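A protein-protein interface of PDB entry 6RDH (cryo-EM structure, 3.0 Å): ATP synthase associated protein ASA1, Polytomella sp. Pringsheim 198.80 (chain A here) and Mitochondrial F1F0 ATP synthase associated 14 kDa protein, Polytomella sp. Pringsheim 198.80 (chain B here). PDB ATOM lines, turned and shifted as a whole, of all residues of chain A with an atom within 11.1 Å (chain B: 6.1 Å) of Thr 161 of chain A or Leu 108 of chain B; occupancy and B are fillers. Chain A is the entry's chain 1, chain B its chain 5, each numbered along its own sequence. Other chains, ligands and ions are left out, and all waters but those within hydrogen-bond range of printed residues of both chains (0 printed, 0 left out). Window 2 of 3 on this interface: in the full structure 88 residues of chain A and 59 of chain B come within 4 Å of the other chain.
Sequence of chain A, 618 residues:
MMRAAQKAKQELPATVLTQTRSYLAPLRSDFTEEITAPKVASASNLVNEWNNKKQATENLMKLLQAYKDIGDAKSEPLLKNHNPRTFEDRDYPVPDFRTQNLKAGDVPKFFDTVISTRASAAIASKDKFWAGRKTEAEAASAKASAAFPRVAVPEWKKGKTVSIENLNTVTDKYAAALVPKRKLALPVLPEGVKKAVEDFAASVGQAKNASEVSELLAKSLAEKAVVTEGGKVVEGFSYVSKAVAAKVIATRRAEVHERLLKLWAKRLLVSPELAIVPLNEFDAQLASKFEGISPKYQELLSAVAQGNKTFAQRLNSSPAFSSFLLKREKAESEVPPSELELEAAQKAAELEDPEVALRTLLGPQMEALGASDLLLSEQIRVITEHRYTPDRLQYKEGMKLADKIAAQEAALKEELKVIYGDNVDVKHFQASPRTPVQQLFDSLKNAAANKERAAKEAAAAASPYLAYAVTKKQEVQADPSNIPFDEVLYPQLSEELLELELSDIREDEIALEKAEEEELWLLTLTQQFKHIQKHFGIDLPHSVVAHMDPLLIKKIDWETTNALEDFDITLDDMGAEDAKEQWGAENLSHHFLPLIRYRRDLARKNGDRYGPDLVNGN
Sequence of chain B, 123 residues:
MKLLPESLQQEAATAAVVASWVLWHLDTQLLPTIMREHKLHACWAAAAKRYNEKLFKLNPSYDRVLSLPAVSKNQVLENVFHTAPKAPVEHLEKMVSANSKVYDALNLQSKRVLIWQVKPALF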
ATOM      1  N   VAL A 153     -28.023 -23.224   2.827  1.00  0.00           N
ATOM      2  CA  VAL A 153     -26.812 -22.766   3.495  1.00  0.00           C
ATOM      3  C   VAL A 153     -26.511 -23.782   4.588  1.00  0.00           C
ATOM      4  O   VAL A 153     -27.419 -24.524   4.987  1.00  0.00           O
ATOM      5  CB  VAL A 153     -26.989 -21.350   4.051  1.00  0.00           C
ATOM      6  CG1 VAL A 153     -27.183 -20.387   2.929  1.00  0.00           C
ATOM      7  CG2 VAL A 153     -28.168 -21.314   4.947  1.00  0.00           C
ATOM      8  N   PRO A 154     -25.271 -23.902   5.058  1.00  0.00           N
ATOM      9  CA  PRO A 154     -24.992 -24.845   6.143  1.00  0.00           C
ATOM     10  C   PRO A 154     -25.611 -24.388   7.451  1.00  0.00           C
ATOM     11  O   PRO A 154     -25.524 -23.218   7.822  1.00  0.00           O
ATOM     12  CB  PRO A 154     -23.466 -24.864   6.215  1.00  0.00           C
ATOM     13  CG  PRO A 154     -23.034 -23.695   5.485  1.00  0.00           C
ATOM     14  CD  PRO A 154     -24.029 -23.440   4.436  1.00  0.00           C
ATOM     15  N   GLU A 155     -26.240 -25.326   8.142  1.00  0.00           N
ATOM     16  CA  GLU A 155     -26.946 -25.049   9.384  1.00  0.00           C
ATOM     17  C   GLU A 155     -25.938 -24.813  10.498  1.00  0.00           C
ATOM     18  O   GLU A 155     -25.291 -25.749  10.974  1.00  0.00           O
ATOM     19  CB  GLU A 155     -27.878 -26.214   9.699  1.00  0.00           C
ATOM     20  CG  GLU A 155     -28.920 -25.965  10.759  1.00  0.00           C
ATOM     21  CD  GLU A 155     -28.526 -26.535  12.094  1.00  0.00           C
ATOM     22  OE1 GLU A 155     -27.699 -27.466  12.124  1.00  0.00           O
ATOM     23  OE2 GLU A 155     -29.070 -26.071  13.111  1.00  0.00           O
ATOM     24  N   TRP A 156     -25.796 -23.555  10.896  1.00  0.00           N
ATOM     25  CA  TRP A 156     -24.883 -23.132  11.943  1.00  0.00           C
ATOM     26  C   TRP A 156     -25.709 -22.545  13.070  1.00  0.00           C
ATOM     27  O   TRP A 156     -26.523 -21.648  12.843  1.00  0.00           O
ATOM     28  CB  TRP A 156     -23.886 -22.109  11.404  1.00  0.00           C
ATOM     29  CG  TRP A 156     -23.066 -21.387  12.417  1.00  0.00           C
ATOM     30  CD1 TRP A 156     -22.535 -21.894  13.557  1.00  0.00           C
ATOM     31  CD2 TRP A 156     -22.649 -20.023  12.357  1.00  0.00           C
ATOM     32  NE1 TRP A 156     -21.835 -20.929  14.224  1.00  0.00           N
ATOM     33  CE2 TRP A 156     -21.895 -19.767  13.506  1.00  0.00           C
ATOM     34  CE3 TRP A 156     -22.853 -18.991  11.447  1.00  0.00           C
ATOM     35  CZ2 TRP A 156     -21.333 -18.530  13.760  1.00  0.00           C
ATOM     36  CZ3 TRP A 156     -22.298 -17.769  11.704  1.00  0.00           C
ATOM     37  CH2 TRP A 156     -21.552 -17.545  12.848  1.00  0.00           C
ATOM     38  N   LYS A 157     -25.492 -23.050  14.278  1.00  0.00           N
ATOM     39  CA  LYS A 157     -26.233 -22.624  15.455  1.00  0.00           C
ATOM     40  C   LYS A 157     -25.603 -21.355  16.030  1.00  0.00           C
ATOM     41  O   LYS A 157     -24.760 -20.713  15.401  1.00  0.00           O
ATOM     42  CB  LYS A 157     -26.276 -23.760  16.461  1.00  0.00           C
ATOM     43  CG  LYS A 157     -27.201 -24.881  16.068  1.00  0.00           C
ATOM     44  CD  LYS A 157     -28.635 -24.413  16.043  1.00  0.00           C
ATOM     45  CE  LYS A 157     -29.585 -25.574  16.264  1.00  0.00           C
ATOM     46  NZ  LYS A 157     -29.309 -26.287  17.540  1.00  0.00           N
ATOM     47  N   LYS A 158     -25.998 -20.972  17.244  1.00  0.00           N
ATOM     48  CA  LYS A 158     -25.558 -19.692  17.789  1.00  0.00           C
ATOM     49  C   LYS A 158     -24.138 -19.761  18.331  1.00  0.00           C
ATOM     50  O   LYS A 158     -23.282 -18.955  17.954  1.00  0.00           O
ATOM     51  CB  LYS A 158     -26.516 -19.227  18.880  1.00  0.00           C
ATOM     52  CG  LYS A 158     -26.175 -17.875  19.468  1.00  0.00           C
ATOM     53  CD  LYS A 158     -26.210 -16.797  18.415  1.00  0.00           C
ATOM     54  CE  LYS A 158     -26.888 -15.542  18.929  1.00  0.00           C
ATOM     55  NZ  LYS A 158     -26.300 -15.082  20.205  1.00  0.00           N
ATOM     56  N   GLY A 159     -23.867 -20.701  19.223  1.00  0.00           N
ATOM     57  CA  GLY A 159     -22.550 -20.775  19.815  1.00  0.00           C
ATOM     58  C   GLY A 159     -21.821 -22.028  19.403  1.00  0.00           C
ATOM     59  O   GLY A 159     -20.632 -22.195  19.681  1.00  0.00           O
ATOM     60  N   LYS A 160     -22.535 -22.914  18.719  1.00  0.00           N
ATOM     61  CA  LYS A 160     -21.981 -24.192  18.298  1.00  0.00           C
ATOM     62  C   LYS A 160     -21.200 -24.032  17.005  1.00  0.00           C
ATOM     63  O   LYS A 160     -20.891 -22.913  16.586  1.00  0.00           O
ATOM     64  CB  LYS A 160     -23.088 -25.229  18.126  1.00  0.00           C
ATOM     65  CG  LYS A 160     -24.168 -25.182  19.194  1.00  0.00           C
ATOM     66  CD  LYS A 160     -23.619 -25.497  20.574  1.00  0.00           C
ATOM     67  CE  LYS A 160     -24.734 -25.579  21.590  1.00  0.00           C
ATOM     68  NZ  LYS A 160     -25.650 -24.416  21.460  1.00  0.00           N
ATOM     69  N   THR A 161     -20.864 -25.140  16.373  1.00  0.00           N
ATOM     70  CA  THR A 161     -20.088 -25.147  15.149  1.00  0.00           C
ATOM     71  C   THR A 161     -20.910 -25.749  14.020  1.00  0.00           C
ATOM     72  O   THR A 161     -22.104 -26.017  14.161  1.00  0.00           O
ATOM     73  CB  THR A 161     -18.801 -25.934  15.343  1.00  0.00           C
ATOM     74  OG1 THR A 161     -19.142 -27.229  15.838  1.00  0.00           O
ATOM     75  CG2 THR A 161     -17.913 -25.233  16.334  1.00  0.00           C
ATOM     76  N   VAL A 162     -20.258 -25.951  12.883  1.00  0.00           N
ATOM     77  CA  VAL A 162     -20.866 -26.609  11.738  1.00  0.00           C
ATOM     78  C   VAL A 162     -19.974 -27.780  11.345  1.00  0.00           C
ATOM     79  O   VAL A 162     -18.744 -27.685  11.400  1.00  0.00           O
ATOM     80  CB  VAL A 162     -21.112 -25.613  10.576  1.00  0.00           C
ATOM     81  CG1 VAL A 162     -19.839 -25.021  10.021  1.00  0.00           C
ATOM     82  CG2 VAL A 162     -21.934 -26.244   9.481  1.00  0.00           C
ATOM     83  N   SER A 163     -20.593 -28.909  11.031  1.00  0.00           N
ATOM     84  CA  SER A 163     -19.869 -30.131  10.732  1.00  0.00           C
ATOM     85  C   SER A 163     -19.741 -30.321   9.231  1.00  0.00           C
ATOM     86  O   SER A 163     -20.511 -29.768   8.449  1.00  0.00           O
ATOM     87  CB  SER A 163     -20.574 -31.332  11.355  1.00  0.00           C
ATOM     88  OG  SER A 163     -21.876 -31.476  10.823  1.00  0.00           O
ATOM     89  N   ILE A 164     -18.755 -31.126   8.832  1.00  0.00           N
ATOM     90  CA  ILE A 164     -18.543 -31.354   7.410  1.00  0.00           C
ATOM     91  C   ILE A 164     -19.610 -32.283   6.850  1.00  0.00           C
ATOM     92  O   ILE A 164     -19.898 -32.240   5.651  1.00  0.00           O
ATOM     93  CB  ILE A 164     -17.119 -31.885   7.156  1.00  0.00           C
ATOM     94  CG1 ILE A 164     -16.733 -31.736   5.688  1.00  0.00           C
ATOM     95  CG2 ILE A 164     -16.983 -33.328   7.576  1.00  0.00           C
ATOM     96  CD1 ILE A 164     -15.281 -31.980   5.419  1.00  0.00           C
ATOM     97  N   GLU A 165     -20.280 -33.059   7.700  1.00  0.00           N
ATOM     98  CA  GLU A 165     -21.367 -33.915   7.253  1.00  0.00           C
ATOM     99  C   GLU A 165     -22.613 -33.138   6.881  1.00  0.00           C
ATOM    100  O   GLU A 165     -23.541 -33.727   6.328  1.00  0.00           O
ATOM    101  CB  GLU A 165     -21.705 -34.942   8.334  1.00  0.00           C
ATOM    102  CG  GLU A 165     -20.630 -35.995   8.557  1.00  0.00           C
ATOM    103  CD  GLU A 165     -19.549 -35.547   9.523  1.00  0.00           C
ATOM    104  OE1 GLU A 165     -19.679 -34.448  10.098  1.00  0.00           O
ATOM    105  OE2 GLU A 165     -18.563 -36.290   9.702  1.00  0.00           O
ATOM    106  N   ASN A 166     -22.659 -31.845   7.175  1.00  0.00           N
ATOM    107  CA  ASN A 166     -23.721 -30.954   6.741  1.00  0.00           C
ATOM    108  C   ASN A 166     -23.295 -30.022   5.625  1.00  0.00           C
ATOM    109  O   ASN A 166     -24.100 -29.719   4.748  1.00  0.00           O
ATOM    110  CB  ASN A 166     -24.219 -30.124   7.918  1.00  0.00           C
ATOM    111  CG  ASN A 166     -25.459 -29.360   7.594  1.00  0.00           C
ATOM    112  OD1 ASN A 166     -26.221 -29.722   6.705  1.00  0.00           O
ATOM    113  ND2 ASN A 166     -25.672 -28.282   8.309  1.00  0.00           N
ATOM    114  N   LEU A 167     -22.044 -29.562   5.632  1.00  0.00           N
ATOM    115  CA  LEU A 167     -21.518 -28.814   4.497  1.00  0.00           C
ATOM    116  C   LEU A 167     -21.500 -29.661   3.234  1.00  0.00           C
ATOM    117  O   LEU A 167     -21.789 -29.159   2.140  1.00  0.00           O
ATOM    118  CB  LEU A 167     -20.116 -28.312   4.818  1.00  0.00           C
ATOM    119  CG  LEU A 167     -20.018 -27.150   5.794  1.00  0.00           C
ATOM    120  CD1 LEU A 167     -18.719 -27.226   6.510  1.00  0.00           C
ATOM    121  CD2 LEU A 167     -20.080 -25.869   5.037  1.00  0.00           C
ATOM    122  N   SER A 463      -8.665 -27.778   1.856  1.00  0.00           N
ATOM    123  CA  SER A 463      -9.473 -28.289   2.952  1.00  0.00           C
ATOM    124  C   SER A 463     -10.310 -29.440   2.415  1.00  0.00           C
ATOM    125  O   SER A 463     -10.534 -29.516   1.210  1.00  0.00           O
ATOM    126  CB  SER A 463     -10.369 -27.186   3.529  1.00  0.00           C
ATOM    127  OG  SER A 463     -11.248 -26.674   2.550  1.00  0.00           O
ATOM    128  N   PRO A 464     -10.762 -30.360   3.276  1.00  0.00           N
ATOM    129  CA  PRO A 464     -11.597 -31.461   2.773  1.00  0.00           C
ATOM    130  C   PRO A 464     -12.959 -31.027   2.291  1.00  0.00           C
ATOM    131  O   PRO A 464     -13.576 -31.761   1.506  1.00  0.00           O
ATOM    132  CB  PRO A 464     -11.711 -32.406   3.976  1.00  0.00           C
ATOM    133  CG  PRO A 464     -11.317 -31.642   5.112  1.00  0.00           C
ATOM    134  CD  PRO A 464     -10.324 -30.628   4.651  1.00  0.00           C
ATOM    135  N   TYR B 103     -16.655 -23.180   6.483  1.00  0.00           N
ATOM    136  CA  TYR B 103     -15.929 -24.356   6.938  1.00  0.00           C
ATOM    137  C   TYR B 103     -14.688 -23.960   7.715  1.00  0.00           C
ATOM    138  O   TYR B 103     -14.446 -24.476   8.808  1.00  0.00           O
ATOM    139  CB  TYR B 103     -15.537 -25.241   5.754  1.00  0.00           C
ATOM    140  CG  TYR B 103     -14.626 -26.380   6.149  1.00  0.00           C
ATOM    141  CD1 TYR B 103     -15.143 -27.525   6.700  1.00  0.00           C
ATOM    142  CD2 TYR B 103     -13.248 -26.308   5.974  1.00  0.00           C
ATOM    143  CE1 TYR B 103     -14.341 -28.551   7.061  1.00  0.00           C
ATOM    144  CE2 TYR B 103     -12.439 -27.324   6.370  1.00  0.00           C
ATOM    145  CZ  TYR B 103     -12.990 -28.442   6.907  1.00  0.00           C
ATOM    146  OH  TYR B 103     -12.177 -29.467   7.290  1.00  0.00           O
ATOM    147  N   ALA B 105     -13.804 -21.314   9.299  1.00  0.00           N
ATOM    148  CA  ALA B 105     -13.899 -20.658  10.587  1.00  0.00           C
ATOM    149  C   ALA B 105     -14.512 -21.525  11.669  1.00  0.00           C
ATOM    150  O   ALA B 105     -14.182 -21.342  12.839  1.00  0.00           O
ATOM    151  CB  ALA B 105     -14.699 -19.372  10.466  1.00  0.00           C
ATOM    152  N   LEU B 106     -15.389 -22.462  11.332  1.00  0.00           N
ATOM    153  CA  LEU B 106     -16.325 -22.988  12.318  1.00  0.00           C
ATOM    154  C   LEU B 106     -16.411 -24.507  12.285  1.00  0.00           C
ATOM    155  O   LEU B 106     -17.498 -25.071  12.363  1.00  0.00           O
ATOM    156  CB  LEU B 106     -17.716 -22.438  12.049  1.00  0.00           C
ATOM    157  CG  LEU B 106     -17.924 -20.947  11.876  1.00  0.00           C
ATOM    158  CD1 LEU B 106     -19.315 -20.724  11.386  1.00  0.00           C
ATOM    159  CD2 LEU B 106     -17.671 -20.213  13.146  1.00  0.00           C
ATOM    160  N   ASN B 107     -15.287 -25.220  12.193  1.00  0.00           N
ATOM    161  CA  ASN B 107     -15.390 -26.665  12.020  1.00  0.00           C
ATOM    162  C   ASN B 107     -14.937 -27.531  13.194  1.00  0.00           C
ATOM    163  O   ASN B 107     -15.488 -28.626  13.352  1.00  0.00           O
ATOM    164  CB  ASN B 107     -14.605 -27.133  10.794  1.00  0.00           C
ATOM    165  CG  ASN B 107     -15.057 -28.483  10.335  1.00  0.00           C
ATOM    166  OD1 ASN B 107     -16.251 -28.748  10.289  1.00  0.00           O
ATOM    167  ND2 ASN B 107     -14.117 -29.385  10.114  1.00  0.00           N
ATOM    168  N   LEU B 108     -13.955 -27.082  13.990  1.00  0.00           N
ATOM    169  CA  LEU B 108     -13.139 -27.774  15.003  1.00  0.00           C
ATOM    170  C   LEU B 108     -12.085 -28.690  14.398  1.00  0.00           C
ATOM    171  O   LEU B 108     -11.213 -29.175  15.120  1.00  0.00           O
ATOM    172  CB  LEU B 108     -13.915 -28.638  16.010  1.00  0.00           C
ATOM    173  CG  LEU B 108     -14.936 -28.174  17.035  1.00  0.00           C
ATOM    174  CD1 LEU B 108     -16.289 -28.562  16.541  1.00  0.00           C
ATOM    175  CD2 LEU B 108     -14.662 -28.810  18.382  1.00  0.00           C
ATOM    176  N   GLN B 109     -12.132 -28.932  13.100  1.00  0.00           N
ATOM    177  CA  GLN B 109     -11.075 -29.670  12.434  1.00  0.00           C
ATOM    178  C   GLN B 109     -10.440 -28.853  11.333  1.00  0.00           C
ATOM    179  O   GLN B 109      -9.487 -29.318  10.704  1.00  0.00           O
ATOM    180  CB  GLN B 109     -11.601 -30.991  11.864  1.00  0.00           C
ATOM    181  CG  GLN B 109     -11.560 -32.139  12.854  1.00  0.00           C
ATOM    182  CD  GLN B 109     -12.870 -32.331  13.592  1.00  0.00           C
ATOM    183  OE1 GLN B 109     -13.933 -32.428  12.981  1.00  0.00           O
ATOM    184  NE2 GLN B 109     -12.800 -32.382  14.916  1.00  0.00           N
ATOM    185  N   SER B 110     -10.954 -27.657  11.083  1.00  0.00           N
ATOM    186  CA  SER B 110     -10.318 -26.736  10.167  1.00  0.00           C
ATOM    187  C   SER B 110      -8.990 -26.278  10.723  1.00  0.00           C
ATOM    188  O   SER B 110      -8.812 -26.158  11.932  1.00  0.00           O
ATOM    189  CB  SER B 110     -11.190 -25.522   9.932  1.00  0.00           C
ATOM    190  OG  SER B 110     -10.398 -24.518   9.345  1.00  0.00           O
ATOM    191  N   VAL B 113      -9.220 -22.545  12.421  1.00  0.00           N
ATOM    192  CA  VAL B 113     -10.524 -22.482  13.070  1.00  0.00           C
ATOM    193  C   VAL B 113     -10.548 -21.312  14.046  1.00  0.00           C
ATOM    194  O   VAL B 113      -9.514 -20.903  14.584  1.00  0.00           O
ATOM    195  CB  VAL B 113     -10.828 -23.838  13.748  1.00  0.00           C
ATOM    196  CG1 VAL B 113      -9.887 -24.109  14.878  1.00  0.00           C
ATOM    197  CG2 VAL B 113     -12.265 -23.949  14.202  1.00  0.00           C
ATOM    198  N   ILE B 115     -12.281 -21.186  16.964  1.00  0.00           N
ATOM    199  CA  ILE B 115     -12.816 -21.496  18.283  1.00  0.00           C
ATOM    200  C   ILE B 115     -11.842 -21.048  19.367  1.00  0.00           C
ATOM    201  O   ILE B 115     -12.260 -20.638  20.452  1.00  0.00           O
ATOM    202  CB  ILE B 115     -13.177 -22.989  18.371  1.00  0.00           C
ATOM    203  CG1 ILE B 115     -13.742 -23.363  19.739  1.00  0.00           C
ATOM    204  CG2 ILE B 115     -11.997 -23.863  18.039  1.00  0.00           C
ATOM    205  CD1 ILE B 115     -14.986 -22.616  20.106  1.00  0.00           C
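Of the 9 printed residues of chain B, 4 touch a printed residue of chain A.
Printed residues of chain B that touch a printed residue of chain A: Tyr 103, Leu 106, Asn 107 and Leu 108.
Along chain B the printed residues that touch a printed residue of chain A span positions 103 to 108.
Of the 17 printed residues of chain A, 8 touch a printed residue of chain B.
Printed residues of chain A that touch a printed residue of chain B: Trp 156, Thr 161, Val 162, Ser 163, Ile 164, Leu 167, Ser 463 and Pro 464.
Hydrophobic or aromatic side chains of chain A within 4 Å of the printed part of chain B: Trp 156, Val 162, Ile 164, Leu 167 and Pro 464.
Among the printed residues, no Asp or Glu carboxylate lies within 4 Å of a Lys or Arg side-chain nitrogen of the other chain.
N of Val 162 of chain A sits at hydrogen-bond distance from O of Leu 106 of chain B.
The backbone carbonyl oxygen (O) of Val 162 of chain A lies close to the side-chain amide oxygen (OD1) of Asn 107 of chain B (2.9 Å).
The indole nitrogen (NE1) of Trp 156 of chain A sits at hydrogen-bond distance from the backbone carbonyl oxygen (O) of Lys 160 of chain A (3.2 Å).
OH of Tyr 103 of chain B sits close to ND2 of Asn 107 of chain B.
Among the printed residues, pairs that only touch across the chains: Trp 156 of chain A with Leu 106 of chain B (3.5 Å), Thr 161 of chain A with Leu 106 of chain B (3.4 Å), Thr 161 of chain A with Leu 108 of chain B (3.2 Å), Ser 163 of chain A with Asn 107 of chain B (3.9 Å), Ile 164 of chain A with Tyr 103 of chain B (3.9 Å), Ile 164 of chain A with Asn 107 of chain B (3.7 Å), Leu 167 of chain A with Tyr 103 of chain B (3.6 Å), Ser 463 of chain A with Tyr 103 of chain B (3.5 Å) and Pro 464 of chain A with Tyr 103 of chain B (3.2 Å).
Printed residues of chain B within 4 Å of Trp 156 of chain A: Leu 106 (3.5 Å).
Of the printed residues of chain B, Thr 161 of chain A touches Leu 106 and Leu 108.
Printed residues of chain B within 4 Å of Ile 164 of chain A: Tyr 103 (3.9 Å) and Asn 107 (3.7 Å).
Glu 165 of chain A touches none of the printed residues of chain B.
Of the printed residues of chain B, Ser 463 of chain A touches Tyr 103 (3.5 Å).
Of the printed residues of chain A, Tyr 103 of chain B touches Ile 164 (3.9 Å), Leu 167 (3.6 Å), Ser 463 (3.5 Å) and Pro 464 (3.2 Å).
Leu 106 of chain B touches just these residues of chain A: Trp 156, Thr 161 and Val 162.
Asn 107 of chain B touches just these residues of chain A: Val 162 (2.9 Å), Ser 163 (3.9 Å) and Ile 164 (3.7 Å).
Leu 108 of chain B touches just one residue of chain A: Thr 161.
No residue of chain A comes within 4 Å of Ser 110 of chain B.
Ile 115 of chain B touches none of the printed residues of chain A.
The nearest residue of chain B that does not touch Thr 161 of chain A is Asn 107 of chain B (4.6 Å).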
